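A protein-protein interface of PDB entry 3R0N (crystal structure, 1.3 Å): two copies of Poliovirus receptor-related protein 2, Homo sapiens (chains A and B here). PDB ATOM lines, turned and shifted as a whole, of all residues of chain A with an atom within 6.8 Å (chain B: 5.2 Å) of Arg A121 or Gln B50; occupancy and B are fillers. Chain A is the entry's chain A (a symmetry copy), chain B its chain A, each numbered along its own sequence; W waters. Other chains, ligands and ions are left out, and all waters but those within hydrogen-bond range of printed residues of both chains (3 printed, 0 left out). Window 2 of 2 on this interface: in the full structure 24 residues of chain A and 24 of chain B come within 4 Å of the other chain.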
ATOM      1  N   ARG A   5     -27.705   9.150  -7.958  1.00  0.00           N
ATOM      2  CA  ARG A   5     -28.497   9.641  -6.846  1.00  0.00           C
ATOM      3  C   ARG A   5     -27.947   8.995  -5.572  1.00  0.00           C
ATOM      4  O   ARG A   5     -27.394   7.885  -5.604  1.00  0.00           O
ATOM      5  CB  ARG A   5     -29.957   9.250  -7.074  1.00  0.00           C
ATOM      6  CG  ARG A   5     -30.968   9.795  -6.096  1.00  0.00           C
ATOM      7  CD  ARG A   5     -32.367   9.161  -6.311  1.00  0.00           C
ATOM      8  NE  ARG A   5     -32.336   7.728  -6.016  1.00  0.00           N
ATOM      9  CZ  ARG A   5     -32.373   7.202  -4.791  1.00  0.00           C
ATOM     10  NH1 ARG A   5     -32.491   7.981  -3.722  1.00  0.00           N
ATOM     11  NH2 ARG A   5     -32.292   5.891  -4.636  1.00  0.00           N
ATOM     12  N   VAL A   6     -28.122   9.676  -4.448  1.00  0.00           N
ATOM     13  CA  VAL A   6     -27.627   9.169  -3.175  1.00  0.00           C
ATOM     14  C   VAL A   6     -28.722   8.434  -2.404  1.00  0.00           C
ATOM     15  O   VAL A   6     -29.738   9.041  -2.017  1.00  0.00           O
ATOM     16  CB  VAL A   6     -27.074  10.331  -2.303  1.00  0.00           C
ATOM     17  CG1 VAL A   6     -26.532   9.805  -0.996  1.00  0.00           C
ATOM     18  CG2 VAL A   6     -25.995  11.080  -3.061  1.00  0.00           C
ATOM     19  N   GLN A   7     -28.503   7.145  -2.174  1.00  0.00           N
ATOM     20  CA  GLN A   7     -29.452   6.308  -1.481  1.00  0.00           C
ATOM     21  C   GLN A   7     -29.109   6.292   0.004  1.00  0.00           C
ATOM     22  O   GLN A   7     -27.993   5.927   0.402  1.00  0.00           O
ATOM     23  CB  GLN A   7     -29.379   4.897  -2.062  1.00  0.00           C
ATOM     24  CG  GLN A   7     -29.993   3.824  -1.226  1.00  0.00           C
ATOM     25  CD  GLN A   7     -31.466   4.003  -1.047  1.00  0.00           C
ATOM     26  OE1 GLN A   7     -32.181   4.541  -1.915  1.00  0.00           O
ATOM     27  NE2 GLN A   7     -31.963   3.508   0.077  1.00  0.00           N
ATOM     28  N   VAL A   8     -30.084   6.688   0.813  1.00  0.00           N
ATOM     29  CA  VAL A   8     -29.965   6.726   2.265  1.00  0.00           C
ATOM     30  C   VAL A   8     -31.268   6.231   2.882  1.00  0.00           C
ATOM     31  O   VAL A   8     -32.261   6.060   2.160  1.00  0.00           O
ATOM     32  CB  VAL A   8     -29.704   8.175   2.802  1.00  0.00           C
ATOM     33  CG1 VAL A   8     -28.354   8.706   2.370  1.00  0.00           C
ATOM     34  CG2 VAL A   8     -30.829   9.137   2.390  1.00  0.00           C
ATOM     35  N   GLN A  41     -21.915  15.950   6.243  1.00  0.00           N
ATOM     36  CA  GLN A  41     -22.136  17.269   6.817  1.00  0.00           C
ATOM     37  C   GLN A  41     -23.339  17.258   7.744  1.00  0.00           C
ATOM     38  O   GLN A  41     -24.242  16.421   7.602  1.00  0.00           O
ATOM     39  CB  GLN A  41     -22.323  18.329   5.728  1.00  0.00           C
ATOM     40  CG  GLN A  41     -21.136  18.483   4.793  1.00  0.00           C
ATOM     41  CD  GLN A  41     -21.514  19.240   3.555  1.00  0.00           C
ATOM     42  OE1 GLN A  41     -22.250  20.246   3.624  1.00  0.00           O
ATOM     43  NE2 GLN A  41     -21.057  18.748   2.401  1.00  0.00           N
ATOM     44  N   THR A 109     -25.978  14.773   6.205  1.00  0.00           N
ATOM     45  CA  THR A 109     -26.045  14.764   4.752  1.00  0.00           C
ATOM     46  C   THR A 109     -24.806  14.103   4.182  1.00  0.00           C
ATOM     47  O   THR A 109     -23.676  14.496   4.517  1.00  0.00           O
ATOM     48  CB  THR A 109     -26.225  16.177   4.206  1.00  0.00           C
ATOM     49  OG1 THR A 109     -27.449  16.683   4.731  1.00  0.00           O
ATOM     50  CG2 THR A 109     -26.280  16.192   2.683  1.00  0.00           C
ATOM     51  N   CYS A 110     -25.029  13.100   3.336  1.00  0.00           N
ATOM     52  CA  CYS A 110     -23.977  12.378   2.635  1.00  0.00           C
ATOM     53  C   CYS A 110     -23.912  12.918   1.220  1.00  0.00           C
ATOM     54  O   CYS A 110     -24.920  12.895   0.498  1.00  0.00           O
ATOM     55  CB  CYS A 110     -24.315  10.893   2.630  1.00  0.00           C
ATOM     56  SG  CYS A 110     -23.119   9.864   1.802  1.00  0.00           S
ATOM     57  N   GLU A 111     -22.736  13.413   0.826  1.00  0.00           N
ATOM     58  CA  GLU A 111     -22.574  14.056  -0.474  1.00  0.00           C
ATOM     59  C   GLU A 111     -21.423  13.465  -1.258  1.00  0.00           C
ATOM     60  O   GLU A 111     -20.317  13.357  -0.745  1.00  0.00           O
ATOM     61  CB  GLU A 111     -22.351  15.558  -0.271  1.00  0.00           C
ATOM     62  CG  GLU A 111     -22.307  16.431  -1.530  1.00  0.00           C
ATOM     63  CD  GLU A 111     -22.573  17.892  -1.148  1.00  0.00           C
ATOM     64  OE1 GLU A 111     -21.594  18.623  -0.911  1.00  0.00           O
ATOM     65  OE2 GLU A 111     -23.763  18.287  -0.989  1.00  0.00           O
ATOM     66  N   PHE A 112     -21.692  13.110  -2.505  1.00  0.00           N
ATOM     67  CA  PHE A 112     -20.657  12.642  -3.421  1.00  0.00           C
ATOM     68  C   PHE A 112     -20.344  13.733  -4.422  1.00  0.00           C
ATOM     69  O   PHE A 112     -21.255  14.260  -5.085  1.00  0.00           O
ATOM     70  CB  PHE A 112     -21.132  11.421  -4.223  1.00  0.00           C
ATOM     71  CG  PHE A 112     -21.330  10.196  -3.399  1.00  0.00           C
ATOM     72  CD1 PHE A 112     -20.346   9.220  -3.345  1.00  0.00           C
ATOM     73  CD2 PHE A 112     -22.508  10.009  -2.683  1.00  0.00           C
ATOM     74  CE1 PHE A 112     -20.549   8.073  -2.590  1.00  0.00           C
ATOM     75  CE2 PHE A 112     -22.703   8.864  -1.941  1.00  0.00           C
ATOM     76  CZ  PHE A 112     -21.723   7.904  -1.887  1.00  0.00           C
ATOM     77  N   SER A 119     -22.133  17.222  -7.967  1.00  0.00           N
ATOM     78  CA  SER A 119     -22.310  16.822  -6.569  1.00  0.00           C
ATOM     79  C   SER A 119     -23.755  16.545  -6.248  1.00  0.00           C
ATOM     80  O   SER A 119     -24.649  17.326  -6.570  1.00  0.00           O
ATOM     81  CB  SER A 119     -21.741  17.855  -5.613  1.00  0.00           C
ATOM     82  OG  SER A 119     -20.362  17.914  -5.825  1.00  0.00           O
ATOM     83  N   VAL A 120     -23.968  15.387  -5.643  1.00  0.00           N
ATOM     84  CA  VAL A 120     -25.307  14.920  -5.294  1.00  0.00           C
ATOM     85  C   VAL A 120     -25.325  14.495  -3.832  1.00  0.00           C
ATOM     86  O   VAL A 120     -24.290  14.080  -3.285  1.00  0.00           O
ATOM     87  CB  VAL A 120     -25.800  13.775  -6.216  1.00  0.00           C
ATOM     88  CG1 VAL A 120     -26.040  14.330  -7.629  1.00  0.00           C
ATOM     89  CG2 VAL A 120     -24.823  12.595  -6.260  1.00  0.00           C
ATOM     90  N   ARG A 121     -26.488  14.592  -3.189  1.00  0.00           N
ATOM     91  CA  ARG A 121     -26.560  14.384  -1.733  1.00  0.00           C
ATOM     92  C   ARG A 121     -27.815  13.675  -1.299  1.00  0.00           C
ATOM     93  O   ARG A 121     -28.812  13.673  -2.021  1.00  0.00           O
ATOM     94  CB  ARG A 121     -26.412  15.704  -0.990  1.00  0.00           C
ATOM     95  CG  ARG A 121     -27.600  16.578  -1.011  1.00  0.00           C
ATOM     96  CD  ARG A 121     -27.250  18.001  -0.591  1.00  0.00           C
ATOM     97  NE  ARG A 121     -26.481  18.651  -1.633  1.00  0.00           N
ATOM     98  CZ  ARG A 121     -27.008  19.174  -2.745  1.00  0.00           C
ATOM     99  NH1 ARG A 121     -28.326  19.156  -2.958  1.00  0.00           N
ATOM    100  NH2 ARG A 121     -26.217  19.701  -3.656  1.00  0.00           N
ATOM    101  N   GLY A 122     -27.757  13.105  -0.099  1.00  0.00           N
ATOM    102  CA  GLY A 122     -28.921  12.507   0.574  1.00  0.00           C
ATOM    103  C   GLY A 122     -28.815  12.772   2.061  1.00  0.00           C
ATOM    104  O   GLY A 122     -27.723  12.869   2.586  1.00  0.00           O
ATOM    105  N   MET A 123     -29.957  12.902   2.730  1.00  0.00           N
ATOM    106  CA  MET A 123     -30.004  13.318   4.133  1.00  0.00           C
ATOM    107  C   MET A 123     -30.732  12.290   5.000  1.00  0.00           C
ATOM    108  O   MET A 123     -31.748  11.724   4.597  1.00  0.00           O
ATOM    109  CB  MET A 123     -30.673  14.691   4.253  1.00  0.00           C
ATOM    110  CG  MET A 123     -30.592  15.290   5.646  1.00  0.00           C
ATOM    111  SD  MET A 123     -31.468  16.841   5.813  1.00  0.00           S
ATOM    112  CE  MET A 123     -33.168  16.286   5.812  1.00  0.00           C
ATOM    113  N   TRP B  40     -20.933  24.028 -10.051  1.00  0.00           N
ATOM    114  CA  TRP B  40     -21.938  25.080 -10.004  1.00  0.00           C
ATOM    115  C   TRP B  40     -23.299  24.440 -10.092  1.00  0.00           C
ATOM    116  O   TRP B  40     -23.557  23.594 -10.975  1.00  0.00           O
ATOM    117  CB  TRP B  40     -21.747  26.064 -11.149  1.00  0.00           C
ATOM    118  CG  TRP B  40     -20.633  27.031 -10.944  1.00  0.00           C
ATOM    119  CD1 TRP B  40     -19.318  26.903 -11.333  1.00  0.00           C
ATOM    120  CD2 TRP B  40     -20.749  28.330 -10.345  1.00  0.00           C
ATOM    121  NE1 TRP B  40     -18.613  28.036 -10.992  1.00  0.00           N
ATOM    122  CE2 TRP B  40     -19.462  28.931 -10.395  1.00  0.00           C
ATOM    123  CE3 TRP B  40     -21.803  29.042  -9.748  1.00  0.00           C
ATOM    124  CZ2 TRP B  40     -19.227  30.228  -9.920  1.00  0.00           C
ATOM    125  CZ3 TRP B  40     -21.567  30.310  -9.274  1.00  0.00           C
ATOM    126  CH2 TRP B  40     -20.292  30.888  -9.341  1.00  0.00           C
ATOM    127  N   GLN B  41     -24.173  24.845  -9.178  1.00  0.00           N
ATOM    128  CA  GLN B  41     -25.515  24.291  -9.081  1.00  0.00           C
ATOM    129  C   GLN B  41     -26.553  25.400  -9.047  1.00  0.00           C
ATOM    130  O   GLN B  41     -26.257  26.535  -8.644  1.00  0.00           O
ATOM    131  CB  GLN B  41     -25.664  23.396  -7.848  1.00  0.00           C
ATOM    132  CG  GLN B  41     -24.727  22.202  -7.824  1.00  0.00           C
ATOM    133  CD  GLN B  41     -24.655  21.594  -6.455  1.00  0.00           C
ATOM    134  OE1 GLN B  41     -25.686  21.454  -5.766  1.00  0.00           O
ATOM    135  NE2 GLN B  41     -23.436  21.265  -6.020  1.00  0.00           N
ATOM    136  N   ARG B  42     -27.766  25.057  -9.466  1.00  0.00           N
ATOM    137  CA  ARG B  42     -28.910  25.960  -9.343  1.00  0.00           C
ATOM    138  C   ARG B  42     -29.737  25.385  -8.202  1.00  0.00           C
ATOM    139  O   ARG B  42     -30.488  24.435  -8.389  1.00  0.00           O
ATOM    140  CB  ARG B  42     -29.672  26.037 -10.670  1.00  0.00           C
ATOM    141  CG  ARG B  42     -28.791  26.653 -11.745  1.00  0.00           C
ATOM    142  CD  ARG B  42     -29.494  26.859 -13.054  1.00  0.00           C
ATOM    143  NE  ARG B  42     -30.367  28.026 -13.022  1.00  0.00           N
ATOM    144  CZ  ARG B  42     -31.093  28.447 -14.053  1.00  0.00           C
ATOM    145  NH1 ARG B  42     -31.098  27.768 -15.216  1.00  0.00           N
ATOM    146  NH2 ARG B  42     -31.831  29.543 -13.906  1.00  0.00           N
ATOM    147  N   PRO B  43     -29.575  25.922  -6.972  1.00  0.00           N
ATOM    148  CA  PRO B  43     -30.159  25.257  -5.793  1.00  0.00           C
ATOM    149  C   PRO B  43     -31.676  25.272  -5.755  1.00  0.00           C
ATOM    150  O   PRO B  43     -32.276  24.513  -4.990  1.00  0.00           O
ATOM    151  CB  PRO B  43     -29.578  26.067  -4.620  1.00  0.00           C
ATOM    152  CG  PRO B  43     -29.357  27.411  -5.204  1.00  0.00           C
ATOM    153  CD  PRO B  43     -28.811  27.125  -6.585  1.00  0.00           C
ATOM    154  N   ALA B  45     -33.487  24.697  -8.497  1.00  0.00           N
ATOM    155  CA  ALA B  45     -33.928  23.786  -9.558  1.00  0.00           C
ATOM    156  C   ALA B  45     -34.473  22.479  -8.987  1.00  0.00           C
ATOM    157  O   ALA B  45     -34.170  22.137  -7.857  1.00  0.00           O
ATOM    158  CB  ALA B  45     -32.773  23.491 -10.515  1.00  0.00           C
ATOM    159  N   PRO B  46     -35.253  21.722  -9.786  1.00  0.00           N
ATOM    160  CA  PRO B  46     -35.582  20.366  -9.346  1.00  0.00           C
ATOM    161  C   PRO B  46     -34.322  19.612  -8.924  1.00  0.00           C
ATOM    162  O   PRO B  46     -33.236  19.797  -9.498  1.00  0.00           O
ATOM    163  CB  PRO B  46     -36.263  19.735 -10.579  1.00  0.00           C
ATOM    164  CG  PRO B  46     -36.816  20.924 -11.338  1.00  0.00           C
ATOM    165  CD  PRO B  46     -35.811  22.021 -11.117  1.00  0.00           C
ATOM    166  N   ALA B  47     -34.466  18.769  -7.921  1.00  0.00           N
ATOM    167  CA  ALA B  47     -33.322  18.247  -7.204  1.00  0.00           C
ATOM    168  C   ALA B  47     -32.343  17.464  -8.091  1.00  0.00           C
ATOM    169  O   ALA B  47     -31.129  17.541  -7.899  1.00  0.00           O
ATOM    170  CB  ALA B  47     -33.778  17.423  -6.001  1.00  0.00           C
ATOM    171  N   ASN B  48     -32.870  16.747  -9.079  1.00  0.00           N
ATOM    172  CA  ASN B  48     -32.059  15.949  -9.988  1.00  0.00           C
ATOM    173  C   ASN B  48     -31.497  16.746 -11.176  1.00  0.00           C
ATOM    174  O   ASN B  48     -30.884  16.151 -12.060  1.00  0.00           O
ATOM    175  CB  ASN B  48     -32.840  14.727 -10.493  1.00  0.00           C
ATOM    176  CG  ASN B  48     -34.118  15.103 -11.209  1.00  0.00           C
ATOM    177  OD1 ASN B  48     -34.894  15.930 -10.733  1.00  0.00           O
ATOM    178  ND2 ASN B  48     -34.355  14.471 -12.348  1.00  0.00           N
ATOM    179  N   HIS B  49     -31.682  18.072 -11.183  1.00  0.00           N
ATOM    180  CA  HIS B  49     -31.199  18.953 -12.260  1.00  0.00           C
ATOM    181  C   HIS B  49     -30.404  20.123 -11.709  1.00  0.00           C
ATOM    182  O   HIS B  49     -30.267  21.155 -12.365  1.00  0.00           O
ATOM    183  CB  HIS B  49     -32.362  19.442 -13.128  1.00  0.00           C
ATOM    184  CG  HIS B  49     -32.959  18.342 -13.931  1.00  0.00           C
ATOM    185  ND1 HIS B  49     -32.372  17.883 -15.092  1.00  0.00           N
ATOM    186  CD2 HIS B  49     -34.033  17.549 -13.709  1.00  0.00           C
ATOM    187  CE1 HIS B  49     -33.072  16.868 -15.566  1.00  0.00           C
ATOM    188  NE2 HIS B  49     -34.094  16.652 -14.754  1.00  0.00           N
ATOM    189  N   GLN B  50     -29.860  19.982 -10.506  1.00  0.00           N
ATOM    190  CA  GLN B  50     -29.152  21.102  -9.894  1.00  0.00           C
ATOM    191  C   GLN B  50     -27.794  21.370 -10.500  1.00  0.00           C
ATOM    192  O   GLN B  50     -27.399  22.515 -10.634  1.00  0.00           O
ATOM    193  CB  GLN B  50     -29.041  20.905  -8.392  1.00  0.00           C
ATOM    194  CG  GLN B  50     -30.387  21.086  -7.729  1.00  0.00           C
ATOM    195  CD  GLN B  50     -30.419  20.735  -6.264  1.00  0.00           C
ATOM    196  OE1 GLN B  50     -29.452  20.202  -5.716  1.00  0.00           O
ATOM    197  NE2 GLN B  50     -31.562  21.009  -5.619  1.00  0.00           N
ATOM    198  N   ASN B  51     -27.050  20.328 -10.861  1.00  0.00           N
ATOM    199  CA  ASN B  51     -25.693  20.553 -11.382  1.00  0.00           C
ATOM    200  C   ASN B  51     -25.721  21.056 -12.813  1.00  0.00           C
ATOM    201  O   ASN B  51     -26.293  20.390 -13.699  1.00  0.00           O
ATOM    202  CB  ASN B  51     -24.870  19.284 -11.312  1.00  0.00           C
ATOM    203  CG  ASN B  51     -24.478  18.931  -9.904  1.00  0.00           C
ATOM    204  OD1 ASN B  51     -23.453  19.406  -9.392  1.00  0.00           O
ATOM    205  ND2 ASN B  51     -25.250  18.062  -9.282  1.00  0.00           N
ATOM    206  N   VAL B  52     -25.103  22.221 -13.039  1.00  0.00           N
ATOM    207  CA  VAL B  52     -25.001  22.780 -14.385  1.00  0.00           C
ATOM    208  C   VAL B  52     -23.562  22.840 -14.921  1.00  0.00           C
ATOM    209  O   VAL B  52     -23.370  22.958 -16.131  1.00  0.00           O
ATOM    210  CB  VAL B  52     -25.675  24.164 -14.513  1.00  0.00           C
ATOM    211  CG1 VAL B  52     -27.173  24.049 -14.179  1.00  0.00           C
ATOM    212  CG2 VAL B  52     -24.989  25.217 -13.629  1.00  0.00           C
ATOM    213  N   GLU B 111     -19.496  25.494  -5.415  1.00  0.00           N
ATOM    214  CA  GLU B 111     -19.090  24.571  -4.359  1.00  0.00           C
ATOM    215  C   GLU B 111     -17.745  23.940  -4.646  1.00  0.00           C
ATOM    216  O   GLU B 111     -17.532  23.402  -5.724  1.00  0.00           O
ATOM    217  CB  GLU B 111     -20.155  23.483  -4.200  1.00  0.00           C
ATOM    218  CG  GLU B 111     -19.979  22.501  -3.036  1.00  0.00           C
ATOM    219  CD  GLU B 111     -21.322  21.829  -2.727  1.00  0.00           C
ATOM    220  OE1 GLU B 111     -21.572  20.740  -3.277  1.00  0.00           O
ATOM    221  OE2 GLU B 111     -22.171  22.432  -2.012  1.00  0.00           O
HETATM  222  O   HOH W   1     -27.437  17.917  -6.499  1.00  0.00           O
HETATM  223  O   HOH W   2     -18.943  19.661  -3.458  1.00  0.00           O
HETATM  224  O   HOH W   3     -18.299  20.450  -5.860  1.00  0.00           O
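The side-chain carboxylate (OE1) of Glu A111 sits close to the side-chain carboxylate (OE1) of Glu B111, at 3.2 Å. The side-chain amide oxygen (OE1) of Gln B41 lies within hydrogen-bond range of the guanidinium group (NH2) of Arg A121, 2.8 Å away. The guanidinium group of Arg A121 sits at hydrogen-bond distance from the side-chain amide oxygen of Gln B50. The side-chain amide nitrogen (ND2) of Asn B51 lies within hydrogen-bond range of the backbone carbonyl oxygen (O) of Ser A119 (2.9 Å).
The backbone carbonyl oxygen (O) of Gln B50 sits at hydrogen-bond distance from the backbone NH (N) of Arg B42, 2.8 Å away. The side-chain carboxylate (OE2) of Glu A111 is in salt-bridge range of the guanidinium group (NE) of Arg A121 (2.8 Å). OE1 of Glu A111 lies within hydrogen-bond range of NE2 of Gln A41, 3.4 Å away. The side-chain carboxylate (OE1) of Glu B111 sits at hydrogen-bond distance from the side-chain amide nitrogen (NE2) of Gln B41, at 3.4 Å.
Ser A119 touches Gln B41. Ser A119 touches Glu B111.
Printed residues of chain B within 4 Å of Arg A121: Gln B41 (2.8 Å) and Gln B50 (3.2 Å). Printed residues of chain A within 4 Å of Gln B50: Arg A121 (3.2 Å). Printed residues of chain B within 4 Å of Glu A111: Glu B111 (3.2 Å). Of the printed residues of chain A, Asn B51 touches Ser A119. The nearest printed residue of chain A that does not touch Gln B41 is Glu A111 (5.9 Å).
Of the 14 printed residues of chain A, 3 touch a printed residue of chain B. Printed residues of chain A that touch a printed residue of chain B: Glu A111, Ser A119 and Arg A121. Along chain A the printed residues that touch a printed residue of chain B span positions 111 to 121. Of the 13 printed residues of chain B, 4 touch a printed residue of chain A. Among the printed residues, 6 pairs touch across the chains. Among the printed residues, no Asp or Glu carboxylate lies within 4 Å of a Lys or Arg side-chain nitrogen of the other chain.
Glu B111 touches its own counterpart, Glu A111. Of the 6 pairs that touch across the chains among the printed residues, 1 has its exchanged pair printed and touching as well.
Water W2 lies within hydrogen-bond range of OE1 of Glu B111 and OG of Ser A119. Water W1 bridges the backbone carbonyl oxygen of Ser A119 (2.9 Å) and the side-chain amide oxygen of Gln B50 (3.1 Å). Water W3 bridges O of Glu B111 (3.1 Å) and OG of Ser A119 (3.3 Å).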
